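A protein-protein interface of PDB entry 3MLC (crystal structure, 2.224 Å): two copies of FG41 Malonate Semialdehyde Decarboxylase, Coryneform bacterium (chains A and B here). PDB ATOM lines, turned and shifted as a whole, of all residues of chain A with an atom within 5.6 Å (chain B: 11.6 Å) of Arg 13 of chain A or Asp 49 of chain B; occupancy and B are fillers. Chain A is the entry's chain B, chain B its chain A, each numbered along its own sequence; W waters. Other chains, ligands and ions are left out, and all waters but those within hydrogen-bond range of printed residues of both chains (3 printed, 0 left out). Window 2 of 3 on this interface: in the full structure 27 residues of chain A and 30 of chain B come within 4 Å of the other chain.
A ring nitrogen (ND1) of His 45 of chain B lies within hydrogen-bond range of the backbone carbonyl oxygen (O) of Leu 42 of chain A, at 3.5 Å.
OD1 of Asp 49 of chain B lies within salt-bridge range of NH1 of Arg 13 of chain A (3.7 Å).
O of Asp 49 of chain B lies within hydrogen-bond range of N of Leu 42 of chain A, at 2.9 Å.
The backbone NH (N) of Gln 40 of chain A sits at hydrogen-bond distance from the backbone carbonyl oxygen (O) of Ile 51 of chain B (2.8 Å).
Water W2 lies within hydrogen-bond range of the guanidinium group (NH1) of Arg 17 of chain A (2.6 Å) and the backbone carbonyl oxygen (O) of Ser 48 of chain B (3.1 Å).
Water W1 bridges the side-chain carboxylate of Asp 49 of chain B (2.8 Å) and the guanidinium group of Arg 16 of chain A (2.8 Å).
Water W3 lies within hydrogen-bond range of the guanidinium group of Arg 17 of chain A (3.0 Å) and the side-chain carboxylate of Glu 53 of chain B (3.1 Å).
Of the 23 printed residues of chain B, 6 touch a printed residue of chain A.
Hydrophobic or aromatic side chains of chain B that line the printed part of chain A: His 45, Ile 50 and Ile 67.
Among the printed residues, Asp or Glu carboxylates within 4 Å of a Lys or Arg side-chain nitrogen of the other chain: Arg 13 of chain A with Asp 49 of chain B.
OD1 of Asp 6 of chain B is in hydrogen-bond range of NE2 of His 45 of chain B (2.7 Å).
N of Asp 6 of chain B sits at hydrogen-bond distance from O of Ile 67 of chain B (2.7 Å).
N of His 45 of chain B sits at hydrogen-bond distance from O of Leu 7 of chain B.
The backbone NH (N) of Ser 9 of chain B lies within hydrogen-bond range of the backbone carbonyl oxygen (O) of His 45 of chain B (2.9 Å).
Of the printed residues of chain B, Arg 13 of chain A touches Asp 49 (3.7 Å).
Of chain A, only Arg 13 (3.7 Å), Gln 40 (3.5 Å), Ile 41 (3.6 Å) and Leu 42 (2.9 Å) come within 4 Å of Asp 49 of chain B.
Ser 12 of chain A touches none of the printed residues of chain B.
No residue of chain B comes within 4 Å of Glu 14 of chain A.
Of chain B, only His 45 (3.3 Å) comes within 4 Å of Thr 43 of chain A.
Of the printed residues of chain B, Gln 40 of chain A touches Asp 49 (3.5 Å), Ile 50 (3.4 Å) and Ile 51 (2.8 Å).
Printed residues of chain A within 4 Å of Ile 67 of chain B: Ile 41 (3.8 Å).
Of the printed residues of chain A, His 45 of chain B touches Ile 41, Leu 42 and Thr 43.
Arg 11 of chain A touches none of the printed residues of chain B.
The nearest residue of chain A that does not touch Asp 49 of chain B is Arg 16 of chain A (5.0 Å).
Asp 49 of chain B touches Gln 40 of chain A (O to O, 3.5 Å).
O of Gln 40 of chain A touches CA of Ile 50 of chain B, at 3.4 Å.
Asp 6 of chain B touches Ile 41 of chain A.
His 45 of chain B touches Ile 41 of chain A (CE1 to CG2, 3.5 Å).
Asp 49 of chain B touches Ile 41 of chain A.
Ile 41 of chain A touches Ile 67 of chain B (CG1 to CD1, 3.8 Å).
Thr 43 of chain A touches His 45 of chain B (OG1 to CE1, 3.3 Å).
1 position is printed for both chains.
Of the 11 pairs that touch across the chains among the printed residues, none has its exchanged pair printed and touching as well.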
ATOM      1  N   ARG A  11     -15.334  -5.183 -21.585  1.00  0.00           N
ATOM      2  CA  ARG A  11     -16.241  -4.052 -21.361  1.00  0.00           C
ATOM      3  C   ARG A  11     -16.617  -3.961 -19.894  1.00  0.00           C
ATOM      4  O   ARG A  11     -16.912  -4.979 -19.252  1.00  0.00           O
ATOM      5  CB  ARG A  11     -17.500  -4.169 -22.217  1.00  0.00           C
ATOM      6  CG  ARG A  11     -17.239  -4.368 -23.697  1.00  0.00           C
ATOM      7  CD  ARG A  11     -18.559  -4.355 -24.461  1.00  0.00           C
ATOM      8  NE  ARG A  11     -18.392  -4.419 -25.909  1.00  0.00           N
ATOM      9  CZ  ARG A  11     -18.156  -3.378 -26.723  1.00  0.00           C
ATOM     10  NH1 ARG A  11     -18.019  -2.141 -26.262  1.00  0.00           N
ATOM     11  NH2 ARG A  11     -18.041  -3.581 -28.024  1.00  0.00           N
ATOM     12  N   SER A  12     -16.593  -2.737 -19.374  1.00  0.00           N
ATOM     13  CA  SER A  12     -16.870  -2.471 -17.979  1.00  0.00           C
ATOM     14  C   SER A  12     -18.323  -2.714 -17.681  1.00  0.00           C
ATOM     15  O   SER A  12     -19.172  -2.632 -18.567  1.00  0.00           O
ATOM     16  CB  SER A  12     -16.526  -1.021 -17.628  1.00  0.00           C
ATOM     17  OG  SER A  12     -17.167  -0.114 -18.514  1.00  0.00           O
ATOM     18  N   ARG A  13     -18.592  -3.013 -16.415  1.00  0.00           N
ATOM     19  CA  ARG A  13     -19.940  -3.180 -15.919  1.00  0.00           C
ATOM     20  C   ARG A  13     -20.833  -1.965 -16.233  1.00  0.00           C
ATOM     21  O   ARG A  13     -22.024  -2.119 -16.526  1.00  0.00           O
ATOM     22  CB  ARG A  13     -19.895  -3.487 -14.418  1.00  0.00           C
ATOM     23  CG  ARG A  13     -19.088  -4.742 -14.085  1.00  0.00           C
ATOM     24  CD  ARG A  13     -19.570  -5.368 -12.774  1.00  0.00           C
ATOM     25  NE  ARG A  13     -19.181  -6.773 -12.607  1.00  0.00           N
ATOM     26  CZ  ARG A  13     -19.864  -7.818 -13.081  1.00  0.00           C
ATOM     27  NH1 ARG A  13     -20.977  -7.637 -13.791  1.00  0.00           N
ATOM     28  NH2 ARG A  13     -19.430  -9.058 -12.852  1.00  0.00           N
ATOM     29  N   GLU A  14     -20.261  -0.763 -16.183  1.00  0.00           N
ATOM     30  CA  GLU A  14     -21.000   0.443 -16.575  1.00  0.00           C
ATOM     31  C   GLU A  14     -21.427   0.446 -18.049  1.00  0.00           C
ATOM     32  O   GLU A  14     -22.564   0.820 -18.349  1.00  0.00           O
ATOM     33  CB  GLU A  14     -20.255   1.740 -16.215  1.00  0.00           C
ATOM     34  CG  GLU A  14     -18.732   1.653 -16.354  1.00  0.00           C
ATOM     35  CD  GLU A  14     -18.118   2.861 -17.050  1.00  0.00           C
ATOM     36  OE1 GLU A  14     -17.210   2.648 -17.893  1.00  0.00           O
ATOM     37  OE2 GLU A  14     -18.541   4.012 -16.756  1.00  0.00           O
ATOM     38  N   GLN A  15     -20.525   0.056 -18.952  1.00  0.00           N
ATOM     39  CA  GLN A  15     -20.879  -0.081 -20.362  1.00  0.00           C
ATOM     40  C   GLN A  15     -21.857  -1.243 -20.602  1.00  0.00           C
ATOM     41  O   GLN A  15     -22.738  -1.125 -21.451  1.00  0.00           O
ATOM     42  CB  GLN A  15     -19.651  -0.213 -21.256  1.00  0.00           C
ATOM     43  CG  GLN A  15     -19.978  -0.059 -22.756  1.00  0.00           C
ATOM     44  CD  GLN A  15     -18.747  -0.135 -23.663  1.00  0.00           C
ATOM     45  OE1 GLN A  15     -18.533   0.731 -24.515  1.00  0.00           O
ATOM     46  NE2 GLN A  15     -17.946  -1.164 -23.486  1.00  0.00           N
ATOM     47  N   ARG A  16     -21.723  -2.334 -19.838  1.00  0.00           N
ATOM     48  CA  ARG A  16     -22.642  -3.466 -19.944  1.00  0.00           C
ATOM     49  C   ARG A  16     -24.098  -3.033 -19.702  1.00  0.00           C
ATOM     50  O   ARG A  16     -25.008  -3.396 -20.468  1.00  0.00           O
ATOM     51  CB  ARG A  16     -22.211  -4.617 -19.018  1.00  0.00           C
ATOM     52  CG  ARG A  16     -20.995  -5.386 -19.527  1.00  0.00           C
ATOM     53  CD  ARG A  16     -20.475  -6.403 -18.522  1.00  0.00           C
ATOM     54  NE  ARG A  16     -19.028  -6.613 -18.659  1.00  0.00           N
ATOM     55  CZ  ARG A  16     -18.313  -7.488 -17.948  1.00  0.00           C
ATOM     56  NH1 ARG A  16     -18.900  -8.275 -17.049  1.00  0.00           N
ATOM     57  NH2 ARG A  16     -17.004  -7.591 -18.143  1.00  0.00           N
ATOM     58  N   ARG A  17     -24.302  -2.213 -18.700  1.00  0.00           N
ATOM     59  CA  ARG A  17     -25.605  -1.728 -18.366  1.00  0.00           C
ATOM     60  C   ARG A  17     -26.094  -0.657 -19.329  1.00  0.00           C
ATOM     61  O   ARG A  17     -27.253  -0.570 -19.649  1.00  0.00           O
ATOM     62  CB  ARG A  17     -25.574  -1.195 -16.947  1.00  0.00           C
ATOM     63  CG  ARG A  17     -26.837  -0.562 -16.489  1.00  0.00           C
ATOM     64  CD  ARG A  17     -28.011  -1.490 -16.564  1.00  0.00           C
ATOM     65  NE  ARG A  17     -29.255  -0.744 -16.539  1.00  0.00           N
ATOM     66  CZ  ARG A  17     -30.150  -0.811 -15.562  1.00  0.00           C
ATOM     67  NH1 ARG A  17     -29.963  -1.601 -14.536  1.00  0.00           N
ATOM     68  NH2 ARG A  17     -31.233  -0.082 -15.610  1.00  0.00           N
ATOM     69  N   ALA A  18     -25.180   0.162 -19.785  1.00  0.00           N
ATOM     70  CA  ALA A  18     -25.523   1.143 -20.759  1.00  0.00           C
ATOM     71  C   ALA A  18     -25.974   0.446 -22.013  1.00  0.00           C
ATOM     72  O   ALA A  18     -26.970   0.786 -22.573  1.00  0.00           O
ATOM     73  CB  ALA A  18     -24.386   2.025 -21.019  1.00  0.00           C
ATOM     74  N   GLN A  40     -34.087  -9.154 -19.473  1.00  0.00           N
ATOM     75  CA  GLN A  40     -32.741  -9.240 -20.073  1.00  0.00           C
ATOM     76  C   GLN A  40     -31.776 -10.132 -19.312  1.00  0.00           C
ATOM     77  O   GLN A  40     -31.748 -10.142 -18.068  1.00  0.00           O
ATOM     78  CB  GLN A  40     -32.130  -7.842 -20.275  1.00  0.00           C
ATOM     79  CG  GLN A  40     -32.991  -6.942 -21.133  1.00  0.00           C
ATOM     80  CD  GLN A  40     -32.509  -5.503 -21.240  1.00  0.00           C
ATOM     81  OE1 GLN A  40     -31.933  -4.945 -20.304  1.00  0.00           O
ATOM     82  NE2 GLN A  40     -32.774  -4.890 -22.388  1.00  0.00           N
ATOM     83  N   ILE A  41     -31.007 -10.915 -20.078  1.00  0.00           N
ATOM     84  CA  ILE A  41     -29.870 -11.680 -19.531  1.00  0.00           C
ATOM     85  C   ILE A  41     -28.600 -11.178 -20.213  1.00  0.00           C
ATOM     86  O   ILE A  41     -28.492 -11.184 -21.433  1.00  0.00           O
ATOM     87  CB  ILE A  41     -30.066 -13.219 -19.667  1.00  0.00           C
ATOM     88  CG1 ILE A  41     -31.390 -13.659 -18.986  1.00  0.00           C
ATOM     89  CG2 ILE A  41     -28.884 -13.972 -19.059  1.00  0.00           C
ATOM     90  CD1 ILE A  41     -32.044 -14.932 -19.544  1.00  0.00           C
ATOM     91  N   LEU A  42     -27.671 -10.681 -19.410  1.00  0.00           N
ATOM     92  CA  LEU A  42     -26.380 -10.206 -19.884  1.00  0.00           C
ATOM     93  C   LEU A  42     -25.365 -11.268 -19.511  1.00  0.00           C
ATOM     94  O   LEU A  42     -25.251 -11.619 -18.353  1.00  0.00           O
ATOM     95  CB  LEU A  42     -26.049  -8.880 -19.189  1.00  0.00           C
ATOM     96  CG  LEU A  42     -25.226  -7.769 -19.877  1.00  0.00           C
ATOM     97  CD1 LEU A  42     -25.769  -7.398 -21.223  1.00  0.00           C
ATOM     98  CD2 LEU A  42     -25.253  -6.544 -18.988  1.00  0.00           C
ATOM     99  N   THR A  43     -24.652 -11.814 -20.493  1.00  0.00           N
ATOM    100  CA  THR A  43     -23.573 -12.757 -20.229  1.00  0.00           C
ATOM    101  C   THR A  43     -22.260 -12.285 -20.871  1.00  0.00           C
ATOM    102  O   THR A  43     -22.161 -12.108 -22.100  1.00  0.00           O
ATOM    103  CB  THR A  43     -23.902 -14.157 -20.774  1.00  0.00           C
ATOM    104  OG1 THR A  43     -25.239 -14.528 -20.414  1.00  0.00           O
ATOM    105  CG2 THR A  43     -22.912 -15.172 -20.258  1.00  0.00           C
ATOM    106  N   ILE B   5     -31.913 -22.520 -17.461  1.00  0.00           N
ATOM    107  CA  ILE B   5     -32.305 -21.851 -16.234  1.00  0.00           C
ATOM    108  C   ILE B   5     -31.244 -20.811 -15.955  1.00  0.00           C
ATOM    109  O   ILE B   5     -30.089 -21.145 -15.678  1.00  0.00           O
ATOM    110  CB  ILE B   5     -32.411 -22.838 -15.028  1.00  0.00           C
ATOM    111  CG1 ILE B   5     -33.510 -23.883 -15.282  1.00  0.00           C
ATOM    112  CG2 ILE B   5     -32.649 -22.068 -13.711  1.00  0.00           C
ATOM    113  CD1 ILE B   5     -33.213 -25.272 -14.728  1.00  0.00           C
ATOM    114  N   ASP B   6     -31.622 -19.546 -16.016  1.00  0.00           N
ATOM    115  CA  ASP B   6     -30.674 -18.497 -15.694  1.00  0.00           C
ATOM    116  C   ASP B   6     -31.080 -17.824 -14.407  1.00  0.00           C
ATOM    117  O   ASP B   6     -32.201 -17.342 -14.275  1.00  0.00           O
ATOM    118  CB  ASP B   6     -30.552 -17.488 -16.833  1.00  0.00           C
ATOM    119  CG  ASP B   6     -29.763 -18.028 -18.001  1.00  0.00           C
ATOM    120  OD1 ASP B   6     -28.597 -17.607 -18.195  1.00  0.00           O
ATOM    121  OD2 ASP B   6     -30.320 -18.850 -18.746  1.00  0.00           O
ATOM    122  N   LEU B   7     -30.166 -17.814 -13.444  1.00  0.00           N
ATOM    123  CA  LEU B   7     -30.450 -17.308 -12.113  1.00  0.00           C
ATOM    124  C   LEU B   7     -29.275 -16.489 -11.578  1.00  0.00           C
ATOM    125  O   LEU B   7     -28.269 -16.295 -12.266  1.00  0.00           O
ATOM    126  CB  LEU B   7     -30.866 -18.450 -11.154  1.00  0.00           C
ATOM    127  CG  LEU B   7     -29.991 -19.681 -10.879  1.00  0.00           C
ATOM    128  CD1 LEU B   7     -30.674 -20.546  -9.858  1.00  0.00           C
ATOM    129  CD2 LEU B   7     -29.756 -20.498 -12.117  1.00  0.00           C
ATOM    130  N   THR B   8     -29.418 -15.977 -10.362  1.00  0.00           N
ATOM    131  CA  THR B   8     -28.393 -15.105  -9.785  1.00  0.00           C
ATOM    132  C   THR B   8     -27.478 -15.895  -8.838  1.00  0.00           C
ATOM    133  O   THR B   8     -27.861 -16.961  -8.361  1.00  0.00           O
ATOM    134  CB  THR B   8     -29.011 -13.861  -9.112  1.00  0.00           C
ATOM    135  OG1 THR B   8     -29.854 -14.277  -8.047  1.00  0.00           O
ATOM    136  CG2 THR B   8     -29.838 -13.036 -10.104  1.00  0.00           C
ATOM    137  N   SER B   9     -26.277 -15.362  -8.590  1.00  0.00           N
ATOM    138  CA  SER B   9     -25.178 -16.080  -7.907  1.00  0.00           C
ATOM    139  C   SER B   9     -25.171 -15.989  -6.369  1.00  0.00           C
ATOM    140  O   SER B   9     -24.299 -16.558  -5.714  1.00  0.00           O
ATOM    141  CB  SER B   9     -23.824 -15.606  -8.447  1.00  0.00           C
ATOM    142  OG  SER B   9     -23.641 -14.219  -8.199  1.00  0.00           O
ATOM    143  N   ASP B  10     -26.150 -15.308  -5.818  1.00  0.00           N
ATOM    144  CA  ASP B  10     -26.427 -15.331  -4.409  1.00  0.00           C
ATOM    145  C   ASP B  10     -27.021 -16.626  -3.934  1.00  0.00           C
ATOM    146  O   ASP B  10     -27.008 -16.917  -2.763  1.00  0.00           O
ATOM    147  CB  ASP B  10     -27.367 -14.206  -4.037  1.00  0.00           C
ATOM    148  CG  ASP B  10     -28.499 -14.061  -4.999  1.00  0.00           C
ATOM    149  OD1 ASP B  10     -28.229 -14.005  -6.190  1.00  0.00           O
ATOM    150  OD2 ASP B  10     -29.654 -13.962  -4.585  1.00  0.00           O
ATOM    151  N   THR B  43     -27.296 -21.484 -15.500  1.00  0.00           N
ATOM    152  CA  THR B  43     -26.312 -20.389 -15.524  1.00  0.00           C
ATOM    153  C   THR B  43     -26.593 -19.342 -14.451  1.00  0.00           C
ATOM    154  O   THR B  43     -27.733 -18.896 -14.284  1.00  0.00           O
ATOM    155  CB  THR B  43     -26.184 -19.755 -16.915  1.00  0.00           C
ATOM    156  OG1 THR B  43     -26.164 -20.793 -17.909  1.00  0.00           O
ATOM    157  CG2 THR B  43     -24.904 -18.941 -17.007  1.00  0.00           C
ATOM    158  N   ALA B  44     -25.544 -18.974 -13.716  1.00  0.00           N
ATOM    159  CA  ALA B  44     -25.650 -18.048 -12.595  1.00  0.00           C
ATOM    160  C   ALA B  44     -24.892 -16.772 -12.932  1.00  0.00           C
ATOM    161  O   ALA B  44     -23.786 -16.827 -13.447  1.00  0.00           O
ATOM    162  CB  ALA B  44     -25.088 -18.688 -11.345  1.00  0.00           C
ATOM    163  N   HIS B  45     -25.515 -15.620 -12.687  1.00  0.00           N
ATOM    164  CA  HIS B  45     -24.936 -14.350 -13.089  1.00  0.00           C
ATOM    165  C   HIS B  45     -24.841 -13.478 -11.839  1.00  0.00           C
ATOM    166  O   HIS B  45     -25.495 -13.756 -10.831  1.00  0.00           O
ATOM    167  CB  HIS B  45     -25.812 -13.653 -14.143  1.00  0.00           C
ATOM    168  CG  HIS B  45     -26.222 -14.532 -15.289  1.00  0.00           C
ATOM    169  ND1 HIS B  45     -25.575 -14.523 -16.507  1.00  0.00           N
ATOM    170  CD2 HIS B  45     -27.224 -15.436 -15.404  1.00  0.00           C
ATOM    171  CE1 HIS B  45     -26.145 -15.402 -17.314  1.00  0.00           C
ATOM    172  NE2 HIS B  45     -27.155 -15.963 -16.673  1.00  0.00           N
ATOM    173  N   ASP B  46     -24.043 -12.414 -11.911  1.00  0.00           N
ATOM    174  CA  ASP B  46     -24.197 -11.340 -10.955  1.00  0.00           C
ATOM    175  C   ASP B  46     -25.678 -10.908 -11.018  1.00  0.00           C
ATOM    176  O   ASP B  46     -26.281 -10.972 -12.088  1.00  0.00           O
ATOM    177  CB  ASP B  46     -23.256 -10.195 -11.310  1.00  0.00           C
ATOM    178  CG  ASP B  46     -23.017  -9.259 -10.146  1.00  0.00           C
ATOM    179  OD1 ASP B  46     -23.909  -8.438  -9.813  1.00  0.00           O
ATOM    180  OD2 ASP B  46     -21.932  -9.339  -9.548  1.00  0.00           O
ATOM    181  N   PRO B  47     -26.295 -10.561  -9.869  1.00  0.00           N
ATOM    182  CA  PRO B  47     -27.638  -9.928  -9.817  1.00  0.00           C
ATOM    183  C   PRO B  47     -27.912  -8.797 -10.850  1.00  0.00           C
ATOM    184  O   PRO B  47     -29.061  -8.647 -11.322  1.00  0.00           O
ATOM    185  CB  PRO B  47     -27.686  -9.356  -8.395  1.00  0.00           C
ATOM    186  CG  PRO B  47     -26.857 -10.302  -7.580  1.00  0.00           C
ATOM    187  CD  PRO B  47     -25.776 -10.842  -8.510  1.00  0.00           C
ATOM    188  N   SER B  48     -26.877  -8.016 -11.172  1.00  0.00           N
ATOM    189  CA  SER B  48     -26.973  -6.889 -12.103  1.00  0.00           C
ATOM    190  C   SER B  48     -27.132  -7.299 -13.567  1.00  0.00           C
ATOM    191  O   SER B  48     -27.667  -6.526 -14.373  1.00  0.00           O
ATOM    192  CB  SER B  48     -25.767  -5.951 -11.936  1.00  0.00           C
ATOM    193  OG  SER B  48     -24.555  -6.672 -12.045  1.00  0.00           O
ATOM    194  N   ASP B  49     -26.693  -8.516 -13.897  1.00  0.00           N
ATOM    195  CA  ASP B  49     -26.795  -9.063 -15.249  1.00  0.00           C
ATOM    196  C   ASP B  49     -28.186  -9.583 -15.633  1.00  0.00           C
ATOM    197  O   ASP B  49     -28.474  -9.726 -16.817  1.00  0.00           O
ATOM    198  CB  ASP B  49     -25.793 -10.203 -15.447  1.00  0.00           C
ATOM    199  CG  ASP B  49     -24.340  -9.749 -15.391  1.00  0.00           C
ATOM    200  OD1 ASP B  49     -24.040  -8.572 -15.712  1.00  0.00           O
ATOM    201  OD2 ASP B  49     -23.486 -10.620 -15.059  1.00  0.00           O
ATOM    202  N   ILE B  50     -29.035  -9.911 -14.659  1.00  0.00           N
ATOM    203  CA  ILE B  50     -30.424 -10.246 -14.989  1.00  0.00           C
ATOM    204  C   ILE B  50     -31.341  -9.123 -14.549  1.00  0.00           C
ATOM    205  O   ILE B  50     -31.416  -8.811 -13.354  1.00  0.00           O
ATOM    206  CB  ILE B  50     -30.930 -11.573 -14.367  1.00  0.00           C
ATOM    207  CG1 ILE B  50     -29.869 -12.660 -14.458  1.00  0.00           C
ATOM    208  CG2 ILE B  50     -32.247 -12.010 -15.049  1.00  0.00           C
ATOM    209  CD1 ILE B  50     -30.426 -14.041 -14.395  1.00  0.00           C
ATOM    210  N   ILE B  51     -31.998  -8.493 -15.522  1.00  0.00           N
ATOM    211  CA  ILE B  51     -33.042  -7.507 -15.271  1.00  0.00           C
ATOM    212  C   ILE B  51     -34.404  -8.096 -15.637  1.00  0.00           C
ATOM    213  O   ILE B  51     -34.668  -8.403 -16.799  1.00  0.00           O
ATOM    214  CB  ILE B  51     -32.848  -6.177 -16.084  1.00  0.00           C
ATOM    215  CG1 ILE B  51     -31.543  -5.463 -15.739  1.00  0.00           C
ATOM    216  CG2 ILE B  51     -34.016  -5.219 -15.801  1.00  0.00           C
ATOM    217  CD1 ILE B  51     -30.336  -5.901 -16.530  1.00  0.00           C
ATOM    218  N   ALA B  52     -35.273  -8.258 -14.646  1.00  0.00           N
ATOM    219  CA  ALA B  52     -36.637  -8.696 -14.912  1.00  0.00           C
ATOM    220  C   ALA B  52     -37.586  -7.835 -14.091  1.00  0.00           C
ATOM    221  O   ALA B  52     -37.762  -8.034 -12.887  1.00  0.00           O
ATOM    222  CB  ALA B  52     -36.808 -10.178 -14.613  1.00  0.00           C
ATOM    223  N   GLU B  53     -38.173  -6.851 -14.756  1.00  0.00           N
ATOM    224  CA  GLU B  53     -39.110  -5.935 -14.122  1.00  0.00           C
ATOM    225  C   GLU B  53     -40.524  -6.534 -14.160  1.00  0.00           C
ATOM    226  O   GLU B  53     -40.683  -7.737 -14.377  1.00  0.00           O
ATOM    227  CB  GLU B  53     -39.007  -4.553 -14.774  1.00  0.00           C
ATOM    228  CG  GLU B  53     -37.592  -3.951 -14.662  1.00  0.00           C
ATOM    229  CD  GLU B  53     -37.445  -2.588 -15.321  1.00  0.00           C
ATOM    230  OE1 GLU B  53     -38.423  -2.105 -15.925  1.00  0.00           O
ATOM    231  OE2 GLU B  53     -36.339  -1.998 -15.242  1.00  0.00           O
ATOM    232  N   SER B  62     -37.651  -9.622  -5.990  1.00  0.00           N
ATOM    233  CA  SER B  62     -36.337  -9.550  -5.375  1.00  0.00           C
ATOM    234  C   SER B  62     -35.290  -9.527  -6.510  1.00  0.00           C
ATOM    235  O   SER B  62     -35.622  -9.818  -7.674  1.00  0.00           O
ATOM    236  CB  SER B  62     -36.118 -10.701  -4.390  1.00  0.00           C
ATOM    237  OG  SER B  62     -35.771 -11.909  -5.035  1.00  0.00           O
ATOM    238  N   PRO B  63     -34.044  -9.112  -6.205  1.00  0.00           N
ATOM    239  CA  PRO B  63     -32.989  -9.265  -7.217  1.00  0.00           C
ATOM    240  C   PRO B  63     -32.627 -10.718  -7.554  1.00  0.00           C
ATOM    241  O   PRO B  63     -31.878 -10.946  -8.508  1.00  0.00           O
ATOM    242  CB  PRO B  63     -31.788  -8.524  -6.605  1.00  0.00           C
ATOM    243  CG  PRO B  63     -32.071  -8.465  -5.144  1.00  0.00           C
ATOM    244  CD  PRO B  63     -33.558  -8.424  -4.990  1.00  0.00           C
ATOM    245  N   SER B  64     -33.150 -11.679  -6.790  1.00  0.00           N
ATOM    246  CA  SER B  64     -32.855 -13.098  -6.990  1.00  0.00           C
ATOM    247  C   SER B  64     -33.831 -13.752  -7.977  1.00  0.00           C
ATOM    248  O   SER B  64     -34.537 -14.699  -7.635  1.00  0.00           O
ATOM    249  CB  SER B  64     -32.903 -13.840  -5.650  1.00  0.00           C
ATOM    250  OG  SER B  64     -31.954 -13.314  -4.743  1.00  0.00           O
ATOM    251  N   VAL B  65     -33.864 -13.234  -9.200  1.00  0.00           N
ATOM    252  CA  VAL B  65     -34.796 -13.701 -10.228  1.00  0.00           C
ATOM    253  C   VAL B  65     -34.315 -14.998 -10.902  1.00  0.00           C
ATOM    254  O   VAL B  65     -33.122 -15.162 -11.155  1.00  0.00           O
ATOM    255  CB  VAL B  65     -35.041 -12.607 -11.280  1.00  0.00           C
ATOM    256  CG1 VAL B  65     -35.873 -11.479 -10.676  1.00  0.00           C
ATOM    257  CG2 VAL B  65     -33.725 -12.044 -11.764  1.00  0.00           C
ATOM    258  N   VAL B  66     -35.255 -15.908 -11.166  1.00  0.00           N
ATOM    259  CA  VAL B  66     -34.978 -17.152 -11.867  1.00  0.00           C
ATOM    260  C   VAL B  66     -35.708 -17.096 -13.204  1.00  0.00           C
ATOM    261  O   VAL B  66     -36.919 -17.013 -13.236  1.00  0.00           O
ATOM    262  CB  VAL B  66     -35.461 -18.392 -11.065  1.00  0.00           C
ATOM    263  CG1 VAL B  66     -35.109 -19.713 -11.786  1.00  0.00           C
ATOM    264  CG2 VAL B  66     -34.881 -18.370  -9.670  1.00  0.00           C
ATOM    265  N   ILE B  67     -34.953 -17.140 -14.302  1.00  0.00           N
ATOM    266  CA  ILE B  67     -35.528 -17.150 -15.636  1.00  0.00           C
ATOM    267  C   ILE B  67     -35.389 -18.544 -16.209  1.00  0.00           C
ATOM    268  O   ILE B  67     -34.294 -19.108 -16.226  1.00  0.00           O
ATOM    269  CB  ILE B  67     -34.881 -16.079 -16.592  1.00  0.00           C
ATOM    270  CG1 ILE B  67     -35.020 -14.672 -15.992  1.00  0.00           C
ATOM    271  CG2 ILE B  67     -35.508 -16.147 -17.989  1.00  0.00           C
ATOM    272  CD1 ILE B  67     -34.642 -13.556 -16.937  1.00  0.00           C
HETATM  273  O   HOH W   1     -21.549  -9.272 -16.873  1.00  0.00           O
HETATM  274  O   HOH W   2     -28.531  -3.653 -13.817  1.00  0.00           O
HETATM  275  O   HOH W   3     -33.421  -1.659 -14.292  1.00  0.00           O
